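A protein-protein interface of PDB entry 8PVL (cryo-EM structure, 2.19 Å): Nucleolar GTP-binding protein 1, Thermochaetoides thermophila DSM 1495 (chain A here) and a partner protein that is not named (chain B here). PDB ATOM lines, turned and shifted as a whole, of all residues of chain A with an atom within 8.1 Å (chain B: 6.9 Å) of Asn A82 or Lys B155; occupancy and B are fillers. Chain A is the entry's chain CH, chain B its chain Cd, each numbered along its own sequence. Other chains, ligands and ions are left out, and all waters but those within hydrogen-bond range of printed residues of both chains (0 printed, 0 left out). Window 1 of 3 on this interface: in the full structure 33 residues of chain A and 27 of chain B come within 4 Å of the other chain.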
ATOM      1  N   LEU A  70      22.762 -35.021 -16.479  1.00  0.00           N
ATOM      2  CA  LEU A  70      22.741 -34.692 -17.901  1.00  0.00           C
ATOM      3  C   LEU A  70      22.093 -35.794 -18.730  1.00  0.00           C
ATOM      4  O   LEU A  70      21.381 -35.512 -19.700  1.00  0.00           O
ATOM      5  CB  LEU A  70      24.163 -34.422 -18.389  1.00  0.00           C
ATOM      6  CG  LEU A  70      24.575 -32.971 -18.642  1.00  0.00           C
ATOM      7  CD1 LEU A  70      24.146 -32.068 -17.509  1.00  0.00           C
ATOM      8  CD2 LEU A  70      26.078 -32.899 -18.828  1.00  0.00           C
ATOM      9  N   PRO A  75      16.772 -33.718 -24.597  1.00  0.00           N
ATOM     10  CA  PRO A  75      17.949 -33.387 -25.424  1.00  0.00           C
ATOM     11  C   PRO A  75      18.200 -31.898 -25.600  1.00  0.00           C
ATOM     12  O   PRO A  75      19.362 -31.495 -25.741  1.00  0.00           O
ATOM     13  CB  PRO A  75      17.626 -34.062 -26.761  1.00  0.00           C
ATOM     14  CG  PRO A  75      16.797 -35.227 -26.386  1.00  0.00           C
ATOM     15  CD  PRO A  75      15.991 -34.824 -25.183  1.00  0.00           C
ATOM     16  N   PHE A  76      17.152 -31.070 -25.574  1.00  0.00           N
ATOM     17  CA  PHE A  76      17.346 -29.624 -25.606  1.00  0.00           C
ATOM     18  C   PHE A  76      18.107 -29.142 -24.379  1.00  0.00           C
ATOM     19  O   PHE A  76      19.076 -28.386 -24.497  1.00  0.00           O
ATOM     20  CB  PHE A  76      15.999 -28.909 -25.705  1.00  0.00           C
ATOM     21  CG  PHE A  76      16.080 -27.438 -25.422  1.00  0.00           C
ATOM     22  CD1 PHE A  76      16.702 -26.583 -26.317  1.00  0.00           C
ATOM     23  CD2 PHE A  76      15.551 -26.911 -24.255  1.00  0.00           C
ATOM     24  CE1 PHE A  76      16.785 -25.231 -26.057  1.00  0.00           C
ATOM     25  CE2 PHE A  76      15.635 -25.560 -23.990  1.00  0.00           C
ATOM     26  CZ  PHE A  76      16.250 -24.718 -24.893  1.00  0.00           C
ATOM     27  N   HIS A  77      17.687 -29.581 -23.189  1.00  0.00           N
ATOM     28  CA  HIS A  77      18.342 -29.138 -21.963  1.00  0.00           C
ATOM     29  C   HIS A  77      19.751 -29.702 -21.849  1.00  0.00           C
ATOM     30  O   HIS A  77      20.664 -29.007 -21.395  1.00  0.00           O
ATOM     31  CB  HIS A  77      17.507 -29.531 -20.747  1.00  0.00           C
ATOM     32  CG  HIS A  77      16.243 -28.742 -20.602  1.00  0.00           C
ATOM     33  ND1 HIS A  77      16.233 -27.367 -20.523  1.00  0.00           N
ATOM     34  CD2 HIS A  77      14.951 -29.135 -20.525  1.00  0.00           C
ATOM     35  CE1 HIS A  77      14.986 -26.946 -20.401  1.00  0.00           C
ATOM     36  NE2 HIS A  77      14.189 -27.999 -20.400  1.00  0.00           N
ATOM     37  N   ARG A  78      19.944 -30.954 -22.270  1.00  0.00           N
ATOM     38  CA  ARG A  78      21.267 -31.569 -22.250  1.00  0.00           C
ATOM     39  C   ARG A  78      22.231 -30.835 -23.175  1.00  0.00           C
ATOM     40  O   ARG A  78      23.356 -30.493 -22.782  1.00  0.00           O
ATOM     41  CB  ARG A  78      21.144 -33.040 -22.645  1.00  0.00           C
ATOM     42  CG  ARG A  78      22.413 -33.854 -22.523  1.00  0.00           C
ATOM     43  CD  ARG A  78      22.141 -35.296 -22.918  1.00  0.00           C
ATOM     44  NE  ARG A  78      23.210 -36.202 -22.518  1.00  0.00           N
ATOM     45  CZ  ARG A  78      23.115 -37.524 -22.543  1.00  0.00           C
ATOM     46  NH1 ARG A  78      22.007 -38.130 -22.934  1.00  0.00           N
ATOM     47  NH2 ARG A  78      24.157 -38.257 -22.159  1.00  0.00           N
ATOM     48  N   ASP A  79      21.791 -30.551 -24.403  1.00  0.00           N
ATOM     49  CA  ASP A  79      22.656 -29.859 -25.350  1.00  0.00           C
ATOM     50  C   ASP A  79      22.899 -28.414 -24.932  1.00  0.00           C
ATOM     51  O   ASP A  79      24.010 -27.904 -25.095  1.00  0.00           O
ATOM     52  CB  ASP A  79      22.063 -29.927 -26.754  1.00  0.00           C
ATOM     53  CG  ASP A  79      22.518 -31.152 -27.516  1.00  0.00           C
ATOM     54  OD1 ASP A  79      22.430 -32.267 -26.962  1.00  0.00           O
ATOM     55  OD2 ASP A  79      22.976 -30.999 -28.666  1.00  0.00           O
ATOM     56  N   LEU A  80      21.883 -27.741 -24.382  1.00  0.00           N
ATOM     57  CA  LEU A  80      22.067 -26.368 -23.920  1.00  0.00           C
ATOM     58  C   LEU A  80      23.016 -26.307 -22.730  1.00  0.00           C
ATOM     59  O   LEU A  80      23.830 -25.381 -22.627  1.00  0.00           O
ATOM     60  CB  LEU A  80      20.719 -25.746 -23.558  1.00  0.00           C
ATOM     61  CG  LEU A  80      20.778 -24.322 -23.002  1.00  0.00           C
ATOM     62  CD1 LEU A  80      21.316 -23.362 -24.048  1.00  0.00           C
ATOM     63  CD2 LEU A  80      19.421 -23.870 -22.499  1.00  0.00           C
ATOM     64  N   MET A  81      22.922 -27.281 -21.821  1.00  0.00           N
ATOM     65  CA  MET A  81      23.867 -27.355 -20.716  1.00  0.00           C
ATOM     66  C   MET A  81      25.280 -27.580 -21.226  1.00  0.00           C
ATOM     67  O   MET A  81      26.224 -26.975 -20.714  1.00  0.00           O
ATOM     68  CB  MET A  81      23.461 -28.460 -19.743  1.00  0.00           C
ATOM     69  CG  MET A  81      22.669 -27.963 -18.547  1.00  0.00           C
ATOM     70  SD  MET A  81      21.715 -29.258 -17.740  1.00  0.00           S
ATOM     71  CE  MET A  81      20.273 -28.334 -17.221  1.00  0.00           C
ATOM     72  N   ASN A  82      25.437 -28.424 -22.254  1.00  0.00           N
ATOM     73  CA  ASN A  82      26.755 -28.634 -22.851  1.00  0.00           C
ATOM     74  C   ASN A  82      27.285 -27.370 -23.525  1.00  0.00           C
ATOM     75  O   ASN A  82      28.494 -27.109 -23.500  1.00  0.00           O
ATOM     76  CB  ASN A  82      26.708 -29.787 -23.852  1.00  0.00           C
ATOM     77  CG  ASN A  82      27.993 -29.919 -24.646  1.00  0.00           C
ATOM     78  OD1 ASN A  82      29.070 -30.089 -24.079  1.00  0.00           O
ATOM     79  ND2 ASN A  82      27.886 -29.832 -25.964  1.00  0.00           N
ATOM     80  N   ILE A  83      26.407 -26.588 -24.153  1.00  0.00           N
ATOM     81  CA  ILE A  83      26.846 -25.346 -24.787  1.00  0.00           C
ATOM     82  C   ILE A  83      27.270 -24.324 -23.736  1.00  0.00           C
ATOM     83  O   ILE A  83      28.302 -23.659 -23.881  1.00  0.00           O
ATOM     84  CB  ILE A  83      25.746 -24.789 -25.714  1.00  0.00           C
ATOM     85  CG1 ILE A  83      25.482 -25.741 -26.879  1.00  0.00           C
ATOM     86  CG2 ILE A  83      26.121 -23.420 -26.249  1.00  0.00           C
ATOM     87  CD1 ILE A  83      26.684 -26.030 -27.730  1.00  0.00           C
ATOM     88  N   LEU A  84      26.491 -24.191 -22.660  1.00  0.00           N
ATOM     89  CA  LEU A  84      26.802 -23.200 -21.632  1.00  0.00           C
ATOM     90  C   LEU A  84      28.062 -23.571 -20.858  1.00  0.00           C
ATOM     91  O   LEU A  84      28.954 -22.737 -20.668  1.00  0.00           O
ATOM     92  CB  LEU A  84      25.618 -23.044 -20.681  1.00  0.00           C
ATOM     93  CG  LEU A  84      24.368 -22.392 -21.268  1.00  0.00           C
ATOM     94  CD1 LEU A  84      23.210 -22.498 -20.295  1.00  0.00           C
ATOM     95  CD2 LEU A  84      24.647 -20.944 -21.627  1.00  0.00           C
ATOM     96  N   TYR A  85      28.151 -24.814 -20.404  1.00  0.00           N
ATOM     97  CA  TYR A  85      29.305 -25.315 -19.673  1.00  0.00           C
ATOM     98  C   TYR A  85      29.737 -26.609 -20.335  1.00  0.00           C
ATOM     99  O   TYR A  85      28.889 -27.407 -20.731  1.00  0.00           O
ATOM    100  CB  TYR A  85      28.966 -25.559 -18.199  1.00  0.00           C
ATOM    101  CG  TYR A  85      27.656 -24.935 -17.770  1.00  0.00           C
ATOM    102  CD1 TYR A  85      27.586 -23.594 -17.419  1.00  0.00           C
ATOM    103  CD2 TYR A  85      26.488 -25.683 -17.734  1.00  0.00           C
ATOM    104  CE1 TYR A  85      26.391 -23.017 -17.037  1.00  0.00           C
ATOM    105  CE2 TYR A  85      25.289 -25.115 -17.354  1.00  0.00           C
ATOM    106  CZ  TYR A  85      25.247 -23.782 -17.005  1.00  0.00           C
ATOM    107  OH  TYR A  85      24.057 -23.210 -16.625  1.00  0.00           O
ATOM    108  N   ASP A  86      31.043 -26.816 -20.476  1.00  0.00           N
ATOM    109  CA  ASP A  86      31.518 -28.027 -21.135  1.00  0.00           C
ATOM    110  C   ASP A  86      31.075 -29.254 -20.347  1.00  0.00           C
ATOM    111  O   ASP A  86      31.351 -29.366 -19.149  1.00  0.00           O
ATOM    112  CB  ASP A  86      33.037 -27.993 -21.279  1.00  0.00           C
ATOM    113  CG  ASP A  86      33.589 -29.257 -21.899  1.00  0.00           C
ATOM    114  OD1 ASP A  86      33.132 -29.627 -23.001  1.00  0.00           O
ATOM    115  OD2 ASP A  86      34.482 -29.879 -21.290  1.00  0.00           O
ATOM    116  N   ALA A  87      30.334 -30.143 -21.020  1.00  0.00           N
ATOM    117  CA  ALA A  87      29.713 -31.281 -20.346  1.00  0.00           C
ATOM    118  C   ALA A  87      30.752 -32.221 -19.755  1.00  0.00           C
ATOM    119  O   ALA A  87      30.511 -32.832 -18.705  1.00  0.00           O
ATOM    120  CB  ALA A  87      28.809 -32.039 -21.317  1.00  0.00           C
ATOM    121  N   ASP A  88      31.912 -32.331 -20.407  1.00  0.00           N
ATOM    122  CA  ASP A  88      33.020 -33.082 -19.833  1.00  0.00           C
ATOM    123  C   ASP A  88      33.475 -32.466 -18.517  1.00  0.00           C
ATOM    124  O   ASP A  88      33.696 -33.185 -17.541  1.00  0.00           O
ATOM    125  CB  ASP A  88      34.180 -33.148 -20.826  1.00  0.00           C
ATOM    126  CG  ASP A  88      33.865 -34.006 -22.035  1.00  0.00           C
ATOM    127  OD1 ASP A  88      33.015 -34.912 -21.920  1.00  0.00           O
ATOM    128  OD2 ASP A  88      34.467 -33.771 -23.103  1.00  0.00           O
ATOM    129  N   HIS A  89      33.582 -31.135 -18.462  1.00  0.00           N
ATOM    130  CA  HIS A  89      33.982 -30.462 -17.228  1.00  0.00           C
ATOM    131  C   HIS A  89      32.927 -30.620 -16.139  1.00  0.00           C
ATOM    132  O   HIS A  89      33.263 -30.825 -14.968  1.00  0.00           O
ATOM    133  CB  HIS A  89      34.253 -28.985 -17.503  1.00  0.00           C
ATOM    134  CG  HIS A  89      35.585 -28.724 -18.131  1.00  0.00           C
ATOM    135  ND1 HIS A  89      35.839 -28.963 -19.464  1.00  0.00           N
ATOM    136  CD2 HIS A  89      36.740 -28.254 -17.607  1.00  0.00           C
ATOM    137  CE1 HIS A  89      37.091 -28.648 -19.735  1.00  0.00           C
ATOM    138  NE2 HIS A  89      37.661 -28.213 -18.626  1.00  0.00           N
ATOM    139  N   PHE A  90      31.650 -30.529 -16.519  1.00  0.00           N
ATOM    140  CA  PHE A  90      30.536 -30.710 -15.589  1.00  0.00           C
ATOM    141  C   PHE A  90      30.581 -32.091 -14.938  1.00  0.00           C
ATOM    142  O   PHE A  90      30.583 -32.221 -13.699  1.00  0.00           O
ATOM    143  CB  PHE A  90      29.233 -30.502 -16.369  1.00  0.00           C
ATOM    144  CG  PHE A  90      28.000 -30.375 -15.522  1.00  0.00           C
ATOM    145  CD1 PHE A  90      27.634 -29.150 -14.993  1.00  0.00           C
ATOM    146  CD2 PHE A  90      27.175 -31.465 -15.307  1.00  0.00           C
ATOM    147  CE1 PHE A  90      26.489 -29.022 -14.233  1.00  0.00           C
ATOM    148  CE2 PHE A  90      26.026 -31.341 -14.552  1.00  0.00           C
ATOM    149  CZ  PHE A  90      25.685 -30.120 -14.011  1.00  0.00           C
ATOM    150  N   TYR A 148      34.203 -23.818  -9.913  1.00  0.00           N
ATOM    151  CA  TYR A 148      33.480 -24.032 -11.162  1.00  0.00           C
ATOM    152  C   TYR A 148      32.016 -24.382 -10.906  1.00  0.00           C
ATOM    153  O   TYR A 148      31.117 -23.850 -11.572  1.00  0.00           O
ATOM    154  CB  TYR A 148      34.175 -25.133 -11.965  1.00  0.00           C
ATOM    155  CG  TYR A 148      33.397 -25.659 -13.146  1.00  0.00           C
ATOM    156  CD1 TYR A 148      33.390 -24.977 -14.353  1.00  0.00           C
ATOM    157  CD2 TYR A 148      32.691 -26.853 -13.063  1.00  0.00           C
ATOM    158  CE1 TYR A 148      32.689 -25.456 -15.437  1.00  0.00           C
ATOM    159  CE2 TYR A 148      31.986 -27.340 -14.141  1.00  0.00           C
ATOM    160  CZ  TYR A 148      31.990 -26.637 -15.327  1.00  0.00           C
ATOM    161  OH  TYR A 148      31.291 -27.114 -16.409  1.00  0.00           O
ATOM    162  N   MET A 231      31.001 -21.498 -35.092  1.00  0.00           N
ATOM    163  CA  MET A 231      30.060 -20.792 -34.237  1.00  0.00           C
ATOM    164  C   MET A 231      30.548 -20.814 -32.797  1.00  0.00           C
ATOM    165  O   MET A 231      31.048 -21.833 -32.314  1.00  0.00           O
ATOM    166  CB  MET A 231      28.670 -21.425 -34.315  1.00  0.00           C
ATOM    167  CG  MET A 231      28.301 -21.937 -35.686  1.00  0.00           C
ATOM    168  SD  MET A 231      26.547 -21.823 -36.078  1.00  0.00           S
ATOM    169  CE  MET A 231      26.423 -20.112 -36.571  1.00  0.00           C
ATOM    170  N   THR A 233      29.650 -20.100 -28.561  1.00  0.00           N
ATOM    171  CA  THR A 233      28.603 -20.632 -27.691  1.00  0.00           C
ATOM    172  C   THR A 233      27.321 -19.811 -27.775  1.00  0.00           C
ATOM    173  O   THR A 233      26.220 -20.367 -27.653  1.00  0.00           O
ATOM    174  CB  THR A 233      29.102 -20.685 -26.248  1.00  0.00           C
ATOM    175  OG1 THR A 233      29.596 -19.397 -25.864  1.00  0.00           O
ATOM    176  CG2 THR A 233      30.220 -21.701 -26.115  1.00  0.00           C
ATOM    177  N   MET A 236      25.542 -20.893 -30.740  1.00  0.00           N
ATOM    178  CA  MET A 236      25.219 -22.300 -30.569  1.00  0.00           C
ATOM    179  C   MET A 236      24.026 -22.512 -29.651  1.00  0.00           C
ATOM    180  O   MET A 236      23.371 -23.548 -29.759  1.00  0.00           O
ATOM    181  CB  MET A 236      26.427 -23.068 -30.036  1.00  0.00           C
ATOM    182  CG  MET A 236      27.240 -23.760 -31.116  1.00  0.00           C
ATOM    183  SD  MET A 236      26.251 -24.247 -32.541  1.00  0.00           S
ATOM    184  CE  MET A 236      25.822 -25.924 -32.095  1.00  0.00           C
ATOM    185  N   THR A 240      21.100 -24.774 -30.943  1.00  0.00           N
ATOM    186  CA  THR A 240      20.588 -25.852 -30.102  1.00  0.00           C
ATOM    187  C   THR A 240      19.071 -25.780 -29.964  1.00  0.00           C
ATOM    188  O   THR A 240      18.380 -26.804 -30.067  1.00  0.00           O
ATOM    189  CB  THR A 240      21.261 -25.784 -28.728  1.00  0.00           C
ATOM    190  OG1 THR A 240      22.646 -26.130 -28.854  1.00  0.00           O
ATOM    191  CG2 THR A 240      20.595 -26.716 -27.729  1.00  0.00           C
ATOM    192  N   GLN B 131      41.375 -40.013 -19.173  1.00  0.00           N
ATOM    193  CA  GLN B 131      40.694 -39.005 -19.987  1.00  0.00           C
ATOM    194  C   GLN B 131      40.283 -37.772 -19.182  1.00  0.00           C
ATOM    195  O   GLN B 131      40.344 -36.649 -19.693  1.00  0.00           O
ATOM    196  CB  GLN B 131      39.470 -39.626 -20.661  1.00  0.00           C
ATOM    197  CG  GLN B 131      38.923 -38.837 -21.844  1.00  0.00           C
ATOM    198  CD  GLN B 131      39.656 -39.116 -23.149  1.00  0.00           C
ATOM    199  OE1 GLN B 131      40.887 -39.135 -23.204  1.00  0.00           O
ATOM    200  NE2 GLN B 131      38.892 -39.344 -24.211  1.00  0.00           N
ATOM    201  N   THR B 135      41.565 -34.034 -19.965  1.00  0.00           N
ATOM    202  CA  THR B 135      40.675 -32.927 -20.299  1.00  0.00           C
ATOM    203  C   THR B 135      40.913 -31.729 -19.392  1.00  0.00           C
ATOM    204  O   THR B 135      40.881 -30.582 -19.850  1.00  0.00           O
ATOM    205  CB  THR B 135      39.214 -33.371 -20.215  1.00  0.00           C
ATOM    206  OG1 THR B 135      39.008 -34.121 -19.013  1.00  0.00           O
ATOM    207  CG2 THR B 135      38.842 -34.224 -21.413  1.00  0.00           C
ATOM    208  N   ARG B 138      44.153 -30.070 -20.410  1.00  0.00           N
ATOM    209  CA  ARG B 138      43.967 -29.312 -21.642  1.00  0.00           C
ATOM    210  C   ARG B 138      43.211 -28.012 -21.387  1.00  0.00           C
ATOM    211  O   ARG B 138      43.631 -26.940 -21.838  1.00  0.00           O
ATOM    212  CB  ARG B 138      43.236 -30.170 -22.673  1.00  0.00           C
ATOM    213  CG  ARG B 138      43.105 -29.529 -24.040  1.00  0.00           C
ATOM    214  CD  ARG B 138      42.050 -30.226 -24.885  1.00  0.00           C
ATOM    215  NE  ARG B 138      42.077 -31.675 -24.726  1.00  0.00           N
ATOM    216  CZ  ARG B 138      41.079 -32.395 -24.235  1.00  0.00           C
ATOM    217  NH1 ARG B 138      39.948 -31.831 -23.843  1.00  0.00           N
ATOM    218  NH2 ARG B 138      41.219 -33.713 -24.131  1.00  0.00           N
ATOM    219  N   GLU B 139      42.095 -28.083 -20.670  1.00  0.00           N
ATOM    220  CA  GLU B 139      41.289 -26.907 -20.344  1.00  0.00           C
ATOM    221  C   GLU B 139      41.031 -26.885 -18.845  1.00  0.00           C
ATOM    222  O   GLU B 139      40.256 -27.726 -18.344  1.00  0.00           O
ATOM    223  CB  GLU B 139      39.966 -26.906 -21.106  1.00  0.00           C
ATOM    224  CG  GLU B 139      40.083 -27.155 -22.600  1.00  0.00           C
ATOM    225  CD  GLU B 139      39.316 -28.384 -23.045  1.00  0.00           C
ATOM    226  OE1 GLU B 139      39.049 -29.260 -22.198  1.00  0.00           O
ATOM    227  OE2 GLU B 139      38.980 -28.475 -24.244  1.00  0.00           O
ATOM    228  N   ARG B 151      36.832 -19.726 -22.873  1.00  0.00           N
ATOM    229  CA  ARG B 151      36.248 -20.698 -23.787  1.00  0.00           C
ATOM    230  C   ARG B 151      35.245 -20.022 -24.711  1.00  0.00           C
ATOM    231  O   ARG B 151      34.354 -19.298 -24.257  1.00  0.00           O
ATOM    232  CB  ARG B 151      35.579 -21.819 -22.992  1.00  0.00           C
ATOM    233  CG  ARG B 151      34.664 -22.730 -23.793  1.00  0.00           C
ATOM    234  CD  ARG B 151      34.029 -23.763 -22.878  1.00  0.00           C
ATOM    235  NE  ARG B 151      33.079 -24.629 -23.566  1.00  0.00           N
ATOM    236  CZ  ARG B 151      31.764 -24.463 -23.550  1.00  0.00           C
ATOM    237  NH1 ARG B 151      31.203 -23.447 -22.917  1.00  0.00           N
ATOM    238  NH2 ARG B 151      30.991 -25.341 -24.183  1.00  0.00           N
ATOM    239  N   ARG B 153      34.488 -21.749 -28.281  1.00  0.00           N
ATOM    240  CA  ARG B 153      33.898 -22.759 -29.142  1.00  0.00           C
ATOM    241  C   ARG B 153      33.522 -23.989 -28.336  1.00  0.00           C
ATOM    242  O   ARG B 153      34.370 -24.531 -27.615  1.00  0.00           O
ATOM    243  CB  ARG B 153      34.866 -23.150 -30.262  1.00  0.00           C
ATOM    244  CG  ARG B 153      35.319 -21.986 -31.119  1.00  0.00           C
ATOM    245  CD  ARG B 153      34.630 -22.003 -32.471  1.00  0.00           C
ATOM    246  NE  ARG B 153      35.267 -21.111 -33.433  1.00  0.00           N
ATOM    247  CZ  ARG B 153      35.100 -19.795 -33.468  1.00  0.00           C
ATOM    248  NH1 ARG B 153      34.312 -19.173 -32.607  1.00  0.00           N
ATOM    249  NH2 ARG B 153      35.737 -19.087 -34.396  1.00  0.00           N
ATOM    250  N   PRO B 154      32.279 -24.447 -28.415  1.00  0.00           N
ATOM    251  CA  PRO B 154      31.896 -25.674 -27.716  1.00  0.00           C
ATOM    252  C   PRO B 154      32.426 -26.914 -28.422  1.00  0.00           C
ATOM    253  O   PRO B 154      32.792 -26.891 -29.598  1.00  0.00           O
ATOM    254  CB  PRO B 154      30.366 -25.635 -27.755  1.00  0.00           C
ATOM    255  CG  PRO B 154      30.056 -24.852 -28.979  1.00  0.00           C
ATOM    256  CD  PRO B 154      31.140 -23.825 -29.110  1.00  0.00           C
ATOM    257  N   LYS B 155      32.461 -28.009 -27.672  1.00  0.00           N
ATOM    258  CA  LYS B 155      32.832 -29.309 -28.215  1.00  0.00           C
ATOM    259  C   LYS B 155      31.568 -30.035 -28.656  1.00  0.00           C
ATOM    260  O   LYS B 155      30.721 -30.381 -27.825  1.00  0.00           O
ATOM    261  CB  LYS B 155      33.598 -30.130 -27.179  1.00  0.00           C
ATOM    262  CG  LYS B 155      33.927 -31.538 -27.633  1.00  0.00           C
ATOM    263  CD  LYS B 155      34.432 -32.385 -26.480  1.00  0.00           C
ATOM    264  CE  LYS B 155      34.564 -33.842 -26.886  1.00  0.00           C
ATOM    265  NZ  LYS B 155      34.894 -34.710 -25.724  1.00  0.00           N
ATOM    266  N   LEU B 156      31.443 -30.270 -29.957  1.00  0.00           N
ATOM    267  CA  LEU B 156      30.240 -30.840 -30.542  1.00  0.00           C
ATOM    268  C   LEU B 156      30.507 -32.250 -31.053  1.00  0.00           C
ATOM    269  O   LEU B 156      31.617 -32.575 -31.482  1.00  0.00           O
ATOM    270  CB  LEU B 156      29.724 -29.965 -31.688  1.00  0.00           C
ATOM    271  CG  LEU B 156      29.496 -28.490 -31.358  1.00  0.00           C
ATOM    272  CD1 LEU B 156      29.097 -27.718 -32.601  1.00  0.00           C
ATOM    273  CD2 LEU B 156      28.447 -28.342 -30.270  1.00  0.00           C
ATOM    274  N   SER B 157      29.472 -33.084 -31.003  1.00  0.00           N
ATOM    275  CA  SER B 157      29.526 -34.439 -31.531  1.00  0.00           C
ATOM    276  C   SER B 157      29.056 -34.516 -32.976  1.00  0.00           C
ATOM    277  O   SER B 157      28.895 -35.619 -33.508  1.00  0.00           O
ATOM    278  CB  SER B 157      28.688 -35.378 -30.659  1.00  0.00           C
ATOM    279  OG  SER B 157      27.473 -34.762 -30.271  1.00  0.00           O
ATOM    280  N   PHE B 158      28.828 -33.372 -33.615  1.00  0.00           N
ATOM    281  CA  PHE B 158      28.364 -33.305 -34.990  1.00  0.00           C
ATOM    282  C   PHE B 158      29.153 -32.226 -35.713  1.00  0.00           C
ATOM    283  O   PHE B 158      29.689 -31.303 -35.094  1.00  0.00           O
ATOM    284  CB  PHE B 158      26.857 -33.011 -35.063  1.00  0.00           C
ATOM    285  CG  PHE B 158      26.399 -31.947 -34.103  1.00  0.00           C
ATOM    286  CD1 PHE B 158      26.451 -30.607 -34.458  1.00  0.00           C
ATOM    287  CD2 PHE B 158      25.918 -32.284 -32.848  1.00  0.00           C
ATOM    288  CE1 PHE B 158      26.037 -29.628 -33.578  1.00  0.00           C
ATOM    289  CE2 PHE B 158      25.503 -31.308 -31.965  1.00  0.00           C
ATOM    290  CZ  PHE B 158      25.566 -29.978 -32.329  1.00  0.00           C
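A ring nitrogen (NE2) of His A89 is in hydrogen-bond range of the backbone carbonyl oxygen (O) of Glu B139 (2.7 Å).
NH2 of Arg B151 is in hydrogen-bond range of O of Asn A82 (3.1 Å).
The guanidinium group of Arg B151 lies within hydrogen-bond range of the backbone carbonyl oxygen of Ile A83 (3.1 Å).
NH1 of Arg B151 is in hydrogen-bond range of O of Leu A84.
ND2 of Asn A82 sits at hydrogen-bond distance from O of Lys B155 (3.4 Å).
OD2 of Asp A88 is in salt-bridge range of NZ of Lys B155 (2.8 Å).
NH1 of Arg B138 lies within salt-bridge range of OE1 of Glu B139 (3.2 Å).
The side-chain amide oxygen (OD1) of Asn A82 is in hydrogen-bond range of the backbone NH (N) of Ala A87 (3.3 Å).
A ring nitrogen (ND1) of His A89 lies within hydrogen-bond range of the side-chain carboxylate (OD2) of Asp A86.
OG1 of Thr A240 is in hydrogen-bond range of O of Met A236 (2.8 Å).
Among the printed residues, pairs that only touch across the chains: Met A231 with Arg B153 (3.6 Å), Met A236 with Pro B154 (3.7 Å), Ile A83 with Pro B154 (3.7 Å), Met A236 with Leu B156 (3.8 Å), Thr A233 with Arg B151 (3.8 Å), Met A231 with Pro B154 (3.8 Å), Thr A233 with Pro B154 (3.8 Å), Ile A83 with Leu B156 (3.9 Å), Asp A86 with Arg B151 (3.9 Å) and Met A236 with Phe B158 (3.996 Å).
Asn A82 touches just these residues of chain B: Arg B151 (3.1 Å) and Lys B155 (3.4 Å).
Of chain A, only Asn A82 and Asp A88 come within 4 Å of Lys B155.
Of the printed residues of chain B, Asp A86 touches Arg B151.
Of the printed residues of chain B, His A89 touches Glu B139.
Printed residues of chain B within 4 Å of Met A231: Arg B153 (3.6 Å) and Pro B154 (3.8 Å).
Printed residues of chain B within 4 Å of Ile A83: Arg B151, Pro B154 and Leu B156.
Arg A78 touches none of the printed residues of chain B.
Of the 11 printed residues of chain B, 7 touch a printed residue of chain A.
Hydrophobic or aromatic side chains of chain B that line the printed part of chain A: Pro B154, Leu B156 and Phe B158.
Among the printed residues, 16 pairs touch across the chains.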
